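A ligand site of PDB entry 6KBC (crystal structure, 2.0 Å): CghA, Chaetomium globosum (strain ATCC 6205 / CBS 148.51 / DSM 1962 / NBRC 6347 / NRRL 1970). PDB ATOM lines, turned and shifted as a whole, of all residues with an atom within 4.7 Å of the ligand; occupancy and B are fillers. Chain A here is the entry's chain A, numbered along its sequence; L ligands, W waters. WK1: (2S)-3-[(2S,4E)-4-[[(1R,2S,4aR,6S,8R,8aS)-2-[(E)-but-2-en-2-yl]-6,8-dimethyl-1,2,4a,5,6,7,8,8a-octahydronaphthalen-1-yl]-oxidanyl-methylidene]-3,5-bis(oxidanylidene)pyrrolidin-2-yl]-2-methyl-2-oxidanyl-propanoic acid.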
ATOM      1  N   THR A  48     -11.401   5.477  -6.459  1.00  0.00           N
ATOM      2  CA  THR A  48     -10.181   6.143  -6.039  1.00  0.00           C
ATOM      3  C   THR A  48      -9.230   5.124  -5.430  1.00  0.00           C
ATOM      4  O   THR A  48      -9.626   4.323  -4.585  1.00  0.00           O
ATOM      5  CB  THR A  48     -10.481   7.265  -5.028  1.00  0.00           C
ATOM      6  OG1 THR A  48     -11.513   8.112  -5.548  1.00  0.00           O
ATOM      7  CG2 THR A  48      -9.224   8.096  -4.772  1.00  0.00           C
ATOM      8  N   LEU A  50      -5.662   5.674  -3.520  1.00  0.00           N
ATOM      9  CA  LEU A  50      -4.825   6.733  -2.986  1.00  0.00           C
ATOM     10  C   LEU A  50      -3.549   6.148  -2.401  1.00  0.00           C
ATOM     11  O   LEU A  50      -3.599   5.164  -1.648  1.00  0.00           O
ATOM     12  CB  LEU A  50      -5.554   7.547  -1.900  1.00  0.00           C
ATOM     13  CG  LEU A  50      -4.802   8.656  -1.158  1.00  0.00           C
ATOM     14  CD1 LEU A  50      -5.785   9.762  -0.749  1.00  0.00           C
ATOM     15  CD2 LEU A  50      -4.033   8.134   0.083  1.00  0.00           C
ATOM     16  N   SER A  65      -3.836  10.443  -6.018  1.00  0.00           N
ATOM     17  CA  SER A  65      -5.085   9.701  -6.098  1.00  0.00           C
ATOM     18  C   SER A  65      -5.268   9.317  -7.559  1.00  0.00           C
ATOM     19  O   SER A  65      -5.264  10.183  -8.435  1.00  0.00           O
ATOM     20  CB  SER A  65      -6.278  10.536  -5.591  1.00  0.00           C
ATOM     21  OG  SER A  65      -6.215  10.661  -4.182  1.00  0.00           O
ATOM     22  N   PHE A  67      -7.829   8.238 -10.117  1.00  0.00           N
ATOM     23  CA  PHE A  67      -9.272   8.420 -10.231  1.00  0.00           C
ATOM     24  C   PHE A  67      -9.823   7.755 -11.478  1.00  0.00           C
ATOM     25  O   PHE A  67      -9.241   7.855 -12.562  1.00  0.00           O
ATOM     26  CB  PHE A  67      -9.625   9.912 -10.292  1.00  0.00           C
ATOM     27  CG  PHE A  67      -9.519  10.643  -8.987  1.00  0.00           C
ATOM     28  CD1 PHE A  67     -10.188  10.187  -7.857  1.00  0.00           C
ATOM     29  CD2 PHE A  67      -8.785  11.813  -8.895  1.00  0.00           C
ATOM     30  CE1 PHE A  67     -10.119  10.890  -6.654  1.00  0.00           C
ATOM     31  CE2 PHE A  67      -8.702  12.515  -7.694  1.00  0.00           C
ATOM     32  CZ  PHE A  67      -9.379  12.051  -6.571  1.00  0.00           C
ATOM     33  N   ALA A  80      -4.252  12.421  -9.682  1.00  0.00           N
ATOM     34  CA  ALA A  80      -4.130  13.748  -9.094  1.00  0.00           C
ATOM     35  C   ALA A  80      -2.974  13.709  -8.102  1.00  0.00           C
ATOM     36  O   ALA A  80      -3.004  12.934  -7.149  1.00  0.00           O
ATOM     37  CB  ALA A  80      -5.417  14.180  -8.396  1.00  0.00           C
ATOM     38  N   ILE A  81      -1.975  14.564  -8.321  1.00  0.00           N
ATOM     39  CA  ILE A  81      -0.718  14.497  -7.596  1.00  0.00           C
ATOM     40  C   ILE A  81      -0.478  15.796  -6.843  1.00  0.00           C
ATOM     41  O   ILE A  81      -0.646  16.885  -7.402  1.00  0.00           O
ATOM     42  CB  ILE A  81       0.473  14.215  -8.529  1.00  0.00           C
ATOM     43  CG1 ILE A  81       0.260  12.912  -9.296  1.00  0.00           C
ATOM     44  CG2 ILE A  81       1.762  14.144  -7.715  1.00  0.00           C
ATOM     45  CD1 ILE A  81       1.037  12.845 -10.598  1.00  0.00           C
ATOM     46  N   ASN A  82      -0.054  15.680  -5.588  1.00  0.00           N
ATOM     47  CA  ASN A  82       0.342  16.836  -4.816  1.00  0.00           C
ATOM     48  C   ASN A  82       1.636  16.522  -4.085  1.00  0.00           C
ATOM     49  O   ASN A  82       1.797  15.440  -3.527  1.00  0.00           O
ATOM     50  CB  ASN A  82      -0.746  17.232  -3.808  1.00  0.00           C
ATOM     51  CG  ASN A  82      -1.972  17.772  -4.483  1.00  0.00           C
ATOM     52  OD1 ASN A  82      -2.027  18.941  -4.817  1.00  0.00           O
ATOM     53  ND2 ASN A  82      -2.964  16.910  -4.718  1.00  0.00           N
ATOM     54  N   HIS A  94      -2.512  17.287 -12.354  1.00  0.00           N
ATOM     55  CA  HIS A  94      -3.244  16.103 -12.773  1.00  0.00           C
ATOM     56  C   HIS A  94      -2.578  15.540 -14.016  1.00  0.00           C
ATOM     57  O   HIS A  94      -2.225  16.284 -14.936  1.00  0.00           O
ATOM     58  CB  HIS A  94      -4.694  16.436 -13.094  1.00  0.00           C
ATOM     59  CG  HIS A  94      -5.482  16.898 -11.905  1.00  0.00           C
ATOM     60  ND1 HIS A  94      -6.796  17.318 -11.995  1.00  0.00           N
ATOM     61  CD2 HIS A  94      -5.150  16.973 -10.595  1.00  0.00           C
ATOM     62  CE1 HIS A  94      -7.227  17.657 -10.789  1.00  0.00           C
ATOM     63  NE2 HIS A  94      -6.251  17.448  -9.922  1.00  0.00           N
ATOM     64  N   TRP A 183     -14.898   4.312   1.803  1.00  0.00           N
ATOM     65  CA  TRP A 183     -13.528   4.774   1.894  1.00  0.00           C
ATOM     66  C   TRP A 183     -12.916   4.067   3.083  1.00  0.00           C
ATOM     67  O   TRP A 183     -13.405   4.187   4.200  1.00  0.00           O
ATOM     68  CB  TRP A 183     -13.449   6.293   2.066  1.00  0.00           C
ATOM     69  CG  TRP A 183     -12.044   6.783   2.126  1.00  0.00           C
ATOM     70  CD1 TRP A 183     -11.111   6.505   3.096  1.00  0.00           C
ATOM     71  CD2 TRP A 183     -11.388   7.617   1.165  1.00  0.00           C
ATOM     72  NE1 TRP A 183      -9.925   7.130   2.796  1.00  0.00           N
ATOM     73  CE2 TRP A 183     -10.066   7.813   1.618  1.00  0.00           C
ATOM     74  CE3 TRP A 183     -11.792   8.228  -0.012  1.00  0.00           C
ATOM     75  CZ2 TRP A 183      -9.148   8.581   0.913  1.00  0.00           C
ATOM     76  CZ3 TRP A 183     -10.889   8.983  -0.712  1.00  0.00           C
ATOM     77  CH2 TRP A 183      -9.568   9.151  -0.253  1.00  0.00           C
ATOM     78  N   SER A 229     -11.383   3.770  -2.249  1.00  0.00           N
ATOM     79  CA  SER A 229     -12.712   4.352  -2.166  1.00  0.00           C
ATOM     80  C   SER A 229     -13.480   4.055  -3.439  1.00  0.00           C
ATOM     81  O   SER A 229     -12.916   3.938  -4.526  1.00  0.00           O
ATOM     82  CB  SER A 229     -12.651   5.859  -1.958  1.00  0.00           C
ATOM     83  OG  SER A 229     -13.939   6.453  -2.006  1.00  0.00           O
ATOM     84  N   LEU A 231     -17.740   5.183  -4.876  1.00  0.00           N
ATOM     85  CA  LEU A 231     -19.060   5.746  -4.645  1.00  0.00           C
ATOM     86  C   LEU A 231     -19.844   5.646  -5.948  1.00  0.00           C
ATOM     87  O   LEU A 231     -19.292   5.963  -7.011  1.00  0.00           O
ATOM     88  CB  LEU A 231     -18.985   7.229  -4.248  1.00  0.00           C
ATOM     89  CG  LEU A 231     -18.567   7.615  -2.851  1.00  0.00           C
ATOM     90  CD1 LEU A 231     -17.042   7.648  -2.794  1.00  0.00           C
ATOM     91  CD2 LEU A 231     -19.171   8.982  -2.551  1.00  0.00           C
ATOM     92  N   TRP A 235     -20.055  12.678  -5.111  1.00  0.00           N
ATOM     93  CA  TRP A 235     -20.038  12.913  -3.677  1.00  0.00           C
ATOM     94  C   TRP A 235     -20.223  14.385  -3.355  1.00  0.00           C
ATOM     95  O   TRP A 235     -20.744  14.727  -2.292  1.00  0.00           O
ATOM     96  CB  TRP A 235     -18.740  12.347  -3.100  1.00  0.00           C
ATOM     97  CG  TRP A 235     -17.536  13.170  -3.320  1.00  0.00           C
ATOM     98  CD1 TRP A 235     -16.693  13.141  -4.402  1.00  0.00           C
ATOM     99  CD2 TRP A 235     -16.997  14.131  -2.413  1.00  0.00           C
ATOM    100  NE1 TRP A 235     -15.677  14.045  -4.231  1.00  0.00           N
ATOM    101  CE2 TRP A 235     -15.841  14.664  -3.009  1.00  0.00           C
ATOM    102  CE3 TRP A 235     -17.384  14.581  -1.154  1.00  0.00           C
ATOM    103  CZ2 TRP A 235     -15.058  15.629  -2.385  1.00  0.00           C
ATOM    104  CZ3 TRP A 235     -16.615  15.548  -0.528  1.00  0.00           C
ATOM    105  CH2 TRP A 235     -15.464  16.060  -1.150  1.00  0.00           C
ATOM    106  N   ALA A 242     -15.487  17.566   3.879  1.00  0.00           N
ATOM    107  CA  ALA A 242     -14.749  16.314   3.835  1.00  0.00           C
ATOM    108  C   ALA A 242     -13.397  16.567   4.489  1.00  0.00           C
ATOM    109  O   ALA A 242     -12.761  17.576   4.185  1.00  0.00           O
ATOM    110  CB  ALA A 242     -14.581  15.802   2.403  1.00  0.00           C
ATOM    111  N   PHE A 244      -9.793  14.605   5.204  1.00  0.00           N
ATOM    112  CA  PHE A 244      -8.796  13.531   5.178  1.00  0.00           C
ATOM    113  C   PHE A 244      -7.709  13.836   6.199  1.00  0.00           C
ATOM    114  O   PHE A 244      -7.230  14.965   6.274  1.00  0.00           O
ATOM    115  CB  PHE A 244      -8.139  13.404   3.803  1.00  0.00           C
ATOM    116  CG  PHE A 244      -7.026  12.379   3.761  1.00  0.00           C
ATOM    117  CD1 PHE A 244      -7.300  11.042   3.516  1.00  0.00           C
ATOM    118  CD2 PHE A 244      -5.704  12.755   3.980  1.00  0.00           C
ATOM    119  CE1 PHE A 244      -6.272  10.076   3.494  1.00  0.00           C
ATOM    120  CE2 PHE A 244      -4.660  11.804   3.963  1.00  0.00           C
ATOM    121  CZ  PHE A 244      -4.947  10.469   3.720  1.00  0.00           C
ATOM    122  N   MET A 257     -11.212   9.673   7.390  1.00  0.00           N
ATOM    123  CA  MET A 257     -11.997  10.219   6.291  1.00  0.00           C
ATOM    124  C   MET A 257     -13.353  10.531   6.921  1.00  0.00           C
ATOM    125  O   MET A 257     -14.096   9.603   7.233  1.00  0.00           O
ATOM    126  CB  MET A 257     -12.128   9.224   5.128  1.00  0.00           C
ATOM    127  CG  MET A 257     -12.796   9.793   3.862  1.00  0.00           C
ATOM    128  SD  MET A 257     -12.464  11.510   3.409  1.00  0.00           S
ATOM    129  CE  MET A 257     -10.864  11.248   2.704  1.00  0.00           C
ATOM    130  N   LEU A 259     -16.977  12.784   6.663  1.00  0.00           N
ATOM    131  CA  LEU A 259     -17.875  13.532   5.794  1.00  0.00           C
ATOM    132  C   LEU A 259     -18.988  14.158   6.622  1.00  0.00           C
ATOM    133  O   LEU A 259     -19.494  13.535   7.558  1.00  0.00           O
ATOM    134  CB  LEU A 259     -18.541  12.634   4.747  1.00  0.00           C
ATOM    135  CG  LEU A 259     -17.556  11.964   3.781  1.00  0.00           C
ATOM    136  CD1 LEU A 259     -18.300  10.914   3.015  1.00  0.00           C
ATOM    137  CD2 LEU A 259     -17.036  13.041   2.839  1.00  0.00           C
ATOM    138  N   TRP A 350      -1.880  22.686  -0.742  1.00  0.00           N
ATOM    139  CA  TRP A 350      -2.670  23.077  -1.890  1.00  0.00           C
ATOM    140  C   TRP A 350      -3.875  23.859  -1.392  1.00  0.00           C
ATOM    141  O   TRP A 350      -4.234  23.804  -0.215  1.00  0.00           O
ATOM    142  CB  TRP A 350      -3.094  21.862  -2.739  1.00  0.00           C
ATOM    143  CG  TRP A 350      -4.161  20.992  -2.136  1.00  0.00           C
ATOM    144  CD1 TRP A 350      -5.520  21.221  -2.117  1.00  0.00           C
ATOM    145  CD2 TRP A 350      -3.960  19.740  -1.485  1.00  0.00           C
ATOM    146  NE1 TRP A 350      -6.163  20.181  -1.496  1.00  0.00           N
ATOM    147  CE2 TRP A 350      -5.236  19.257  -1.089  1.00  0.00           C
ATOM    148  CE3 TRP A 350      -2.822  18.966  -1.202  1.00  0.00           C
ATOM    149  CZ2 TRP A 350      -5.393  18.050  -0.419  1.00  0.00           C
ATOM    150  CZ3 TRP A 350      -2.993  17.760  -0.530  1.00  0.00           C
ATOM    151  CH2 TRP A 350      -4.276  17.310  -0.150  1.00  0.00           C
ATOM    152  N   LYS A 352      -7.536  25.263  -3.477  1.00  0.00           N
ATOM    153  CA  LYS A 352      -8.254  25.578  -4.691  1.00  0.00           C
ATOM    154  C   LYS A 352      -9.730  25.768  -4.380  1.00  0.00           C
ATOM    155  O   LYS A 352     -10.264  25.118  -3.475  1.00  0.00           O
ATOM    156  CB  LYS A 352      -8.065  24.487  -5.745  1.00  0.00           C
ATOM    157  CG  LYS A 352      -8.626  23.149  -5.372  1.00  0.00           C
ATOM    158  CD  LYS A 352      -8.397  22.154  -6.513  1.00  0.00           C
ATOM    159  CE  LYS A 352      -8.974  20.801  -6.145  1.00  0.00           C
ATOM    160  NZ  LYS A 352      -8.788  19.774  -7.212  1.00  0.00           N
ATOM    161  N   ASN A 364     -10.904  23.707  -1.145  1.00  0.00           N
ATOM    162  CA  ASN A 364     -10.284  22.411  -0.957  1.00  0.00           C
ATOM    163  C   ASN A 364      -8.826  22.717  -0.629  1.00  0.00           C
ATOM    164  O   ASN A 364      -8.094  23.239  -1.472  1.00  0.00           O
ATOM    165  CB  ASN A 364     -10.431  21.565  -2.232  1.00  0.00           C
ATOM    166  CG  ASN A 364      -9.685  20.225  -2.146  1.00  0.00           C
ATOM    167  OD1 ASN A 364      -8.967  19.941  -1.185  1.00  0.00           O
ATOM    168  ND2 ASN A 364      -9.885  19.394  -3.169  1.00  0.00           N
ATOM    169  N   GLY A 389      -6.475  16.959   4.382  1.00  0.00           N
ATOM    170  CA  GLY A 389      -7.138  17.460   3.202  1.00  0.00           C
ATOM    171  C   GLY A 389      -8.493  17.919   3.677  1.00  0.00           C
ATOM    172  O   GLY A 389      -9.253  17.117   4.233  1.00  0.00           O
ATOM    173  N   VAL A 391     -11.907  19.749   2.736  1.00  0.00           N
ATOM    174  CA  VAL A 391     -12.736  20.093   1.593  1.00  0.00           C
ATOM    175  C   VAL A 391     -14.059  20.662   2.081  1.00  0.00           C
ATOM    176  O   VAL A 391     -14.702  20.102   2.972  1.00  0.00           O
ATOM    177  CB  VAL A 391     -12.968  18.893   0.663  1.00  0.00           C
ATOM    178  CG1 VAL A 391     -13.665  19.382  -0.612  1.00  0.00           C
ATOM    179  CG2 VAL A 391     -11.635  18.173   0.350  1.00  0.00           C
HETATM  180  O   WK1 L   1      -6.794  18.233  -7.536  1.00  0.00           O
HETATM  181  C17 WK1 L   1      -6.213  17.731  -6.613  1.00  0.00           C
HETATM  182  O1  WK1 L   1      -5.034  17.545  -6.616  1.00  0.00           O
HETATM  183  C19 WK1 L   1      -6.958  17.336  -5.393  1.00  0.00           C
HETATM  184  O2  WK1 L   1      -8.283  17.724  -5.433  1.00  0.00           O
HETATM  185  C18 WK1 L   1      -6.357  18.040  -4.223  1.00  0.00           C
HETATM  186  C20 WK1 L   1      -6.849  15.838  -5.389  1.00  0.00           C
HETATM  187  C22 WK1 L   1      -7.195  15.284  -4.067  1.00  0.00           C
HETATM  188  N   WK1 L   1      -6.966  13.872  -3.840  1.00  0.00           N
HETATM  189  C21 WK1 L   1      -8.029  13.341  -3.248  1.00  0.00           C
HETATM  190  O5  WK1 L   1      -8.080  12.079  -2.900  1.00  0.00           O
HETATM  191  C23 WK1 L   1      -8.545  15.467  -3.596  1.00  0.00           C
HETATM  192  O4  WK1 L   1      -9.220  16.595  -3.607  1.00  0.00           O
HETATM  193  C24 WK1 L   1      -9.134  14.294  -3.037  1.00  0.00           C
HETATM  194  C16 WK1 L   1     -10.458  14.162  -2.441  1.00  0.00           C
HETATM  195  O3  WK1 L   1     -11.192  15.202  -2.404  1.00  0.00           O
HETATM  196  C9  WK1 L   1     -10.865  12.904  -1.797  1.00  0.00           C
HETATM  197  C8  WK1 L   1     -10.254  13.102  -0.387  1.00  0.00           C
HETATM  198  C12 WK1 L   1      -8.879  13.745  -0.263  1.00  0.00           C
HETATM  199  C13 WK1 L   1      -7.773  13.034  -0.164  1.00  0.00           C
HETATM  200  C90 WK1 L   1      -6.440  13.692  -0.047  1.00  0.00           C
HETATM  201  C14 WK1 L   1      -8.752  15.227  -0.255  1.00  0.00           C
HETATM  202  C7  WK1 L   1     -11.136  13.911   0.504  1.00  0.00           C
HETATM  203  C6  WK1 L   1     -12.391  13.546   0.655  1.00  0.00           C
HETATM  204  C3  WK1 L   1     -12.906  12.522  -0.304  1.00  0.00           C
HETATM  205  C4  WK1 L   1     -12.374  12.684  -1.713  1.00  0.00           C
HETATM  206  C5  WK1 L   1     -12.741  11.419  -2.476  1.00  0.00           C
HETATM  207  C11 WK1 L   1     -12.413  11.584  -3.920  1.00  0.00           C
HETATM  208  C2  WK1 L   1     -14.396  12.285  -0.292  1.00  0.00           C
HETATM  209  C1  WK1 L   1     -14.583  10.915  -0.862  1.00  0.00           C
HETATM  210  C10 WK1 L   1     -15.965  10.366  -0.757  1.00  0.00           C
HETATM  211  C   WK1 L   1     -14.184  10.983  -2.305  1.00  0.00           C
HETATM  212  O   HOH W   1      -9.746  16.752  -7.962  1.00  0.00           O
HETATM  213  O   HOH W   2      -3.076  17.891  -8.461  1.00  0.00           O
HETATM  214  O   HOH W   3      -4.350  12.288  -3.159  1.00  0.00           O
HETATM  215  O   HOH W   4      -3.715  14.116  -4.814  1.00  0.00           O
HETATM  216  O   HOH W   5      -4.268  20.362  -5.949  1.00  0.00           O
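An oxygen (O) of the ligand lies within salt-bridge range of the side-chain amino group (NZ) of Lys 352 (2.5 Å). A ring nitrogen (NE2) of His 94 lies within hydrogen-bond range of an oxygen (O) of the ligand, at 2.6 Å. OG of Ser 65 sits at hydrogen-bond distance from O5 of the ligand, at 2.7 Å. ND2 of Asn 82 lies within hydrogen-bond range of O1 of the ligand, at 2.9 Å. ND2 of Asn 364 is in hydrogen-bond range of O4 of the ligand, 2.9 Å away.
The backbone carbonyl oxygen of Lys 352 lies within hydrogen-bond range of the backbone NH of Asn 364 (2.8 Å). N of Ala 80 sits at hydrogen-bond distance from O of Ser 65, at 2.8 Å. The side-chain amide oxygen (OD1) of Asn 364 sits at hydrogen-bond distance from the indole nitrogen (NE1) of Trp 350, 2.8 Å away. O of Ala 242 lies within hydrogen-bond range of N of Val 391, 2.7 Å away. The backbone NH of Thr 48 lies within hydrogen-bond range of the backbone carbonyl oxygen of Ser 229 (2.9 Å).
Merely in contact with the ligand: Thr 48 (3.9 Å), Leu 50 (3.9 Å), Phe 67 (3.6 Å), Ala 80 (3.7 Å), Trp 183 (3.5 Å), Leu 231 (3.6 Å), Trp 235 (3.8 Å), Ala 242 (3.6 Å), Met 257 (3.4 Å) and Trp 350 (3.5 Å). Hydrophobic or aromatic side chains that line the ligand: Leu 50, Phe 67, Ala 80, His 94, Trp 183, Leu 231, Trp 235, Ala 242, Met 257 and Trp 350. Of the 21 residues printed, 15 come within 4 Å of the ligand. The nearest printed residue that does not touch the ligand is Phe 244 (4.001 Å).
Water W2 bridges an oxygen (O1) of the ligand (2.7 Å) and the backbone carbonyl oxygen (O) of Ile 81 (2.8 Å). Water W5 bridges OD1 of Asn 82 (2.9 Å) and O1 of the ligand (3.0 Å). Water W1 lies within hydrogen-bond range of O2 of the ligand and NZ of Lys 352. Water W3 lies within hydrogen-bond range of OG of Ser 65 (2.7 Å) and N of the ligand (3.1 Å). Water W4 lies within hydrogen-bond range of the backbone carbonyl oxygen of Ala 80 (2.7 Å), the side-chain amide nitrogen of Asn 82 (2.9 Å) and a nitrogen (N) of the ligand (3.4 Å).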
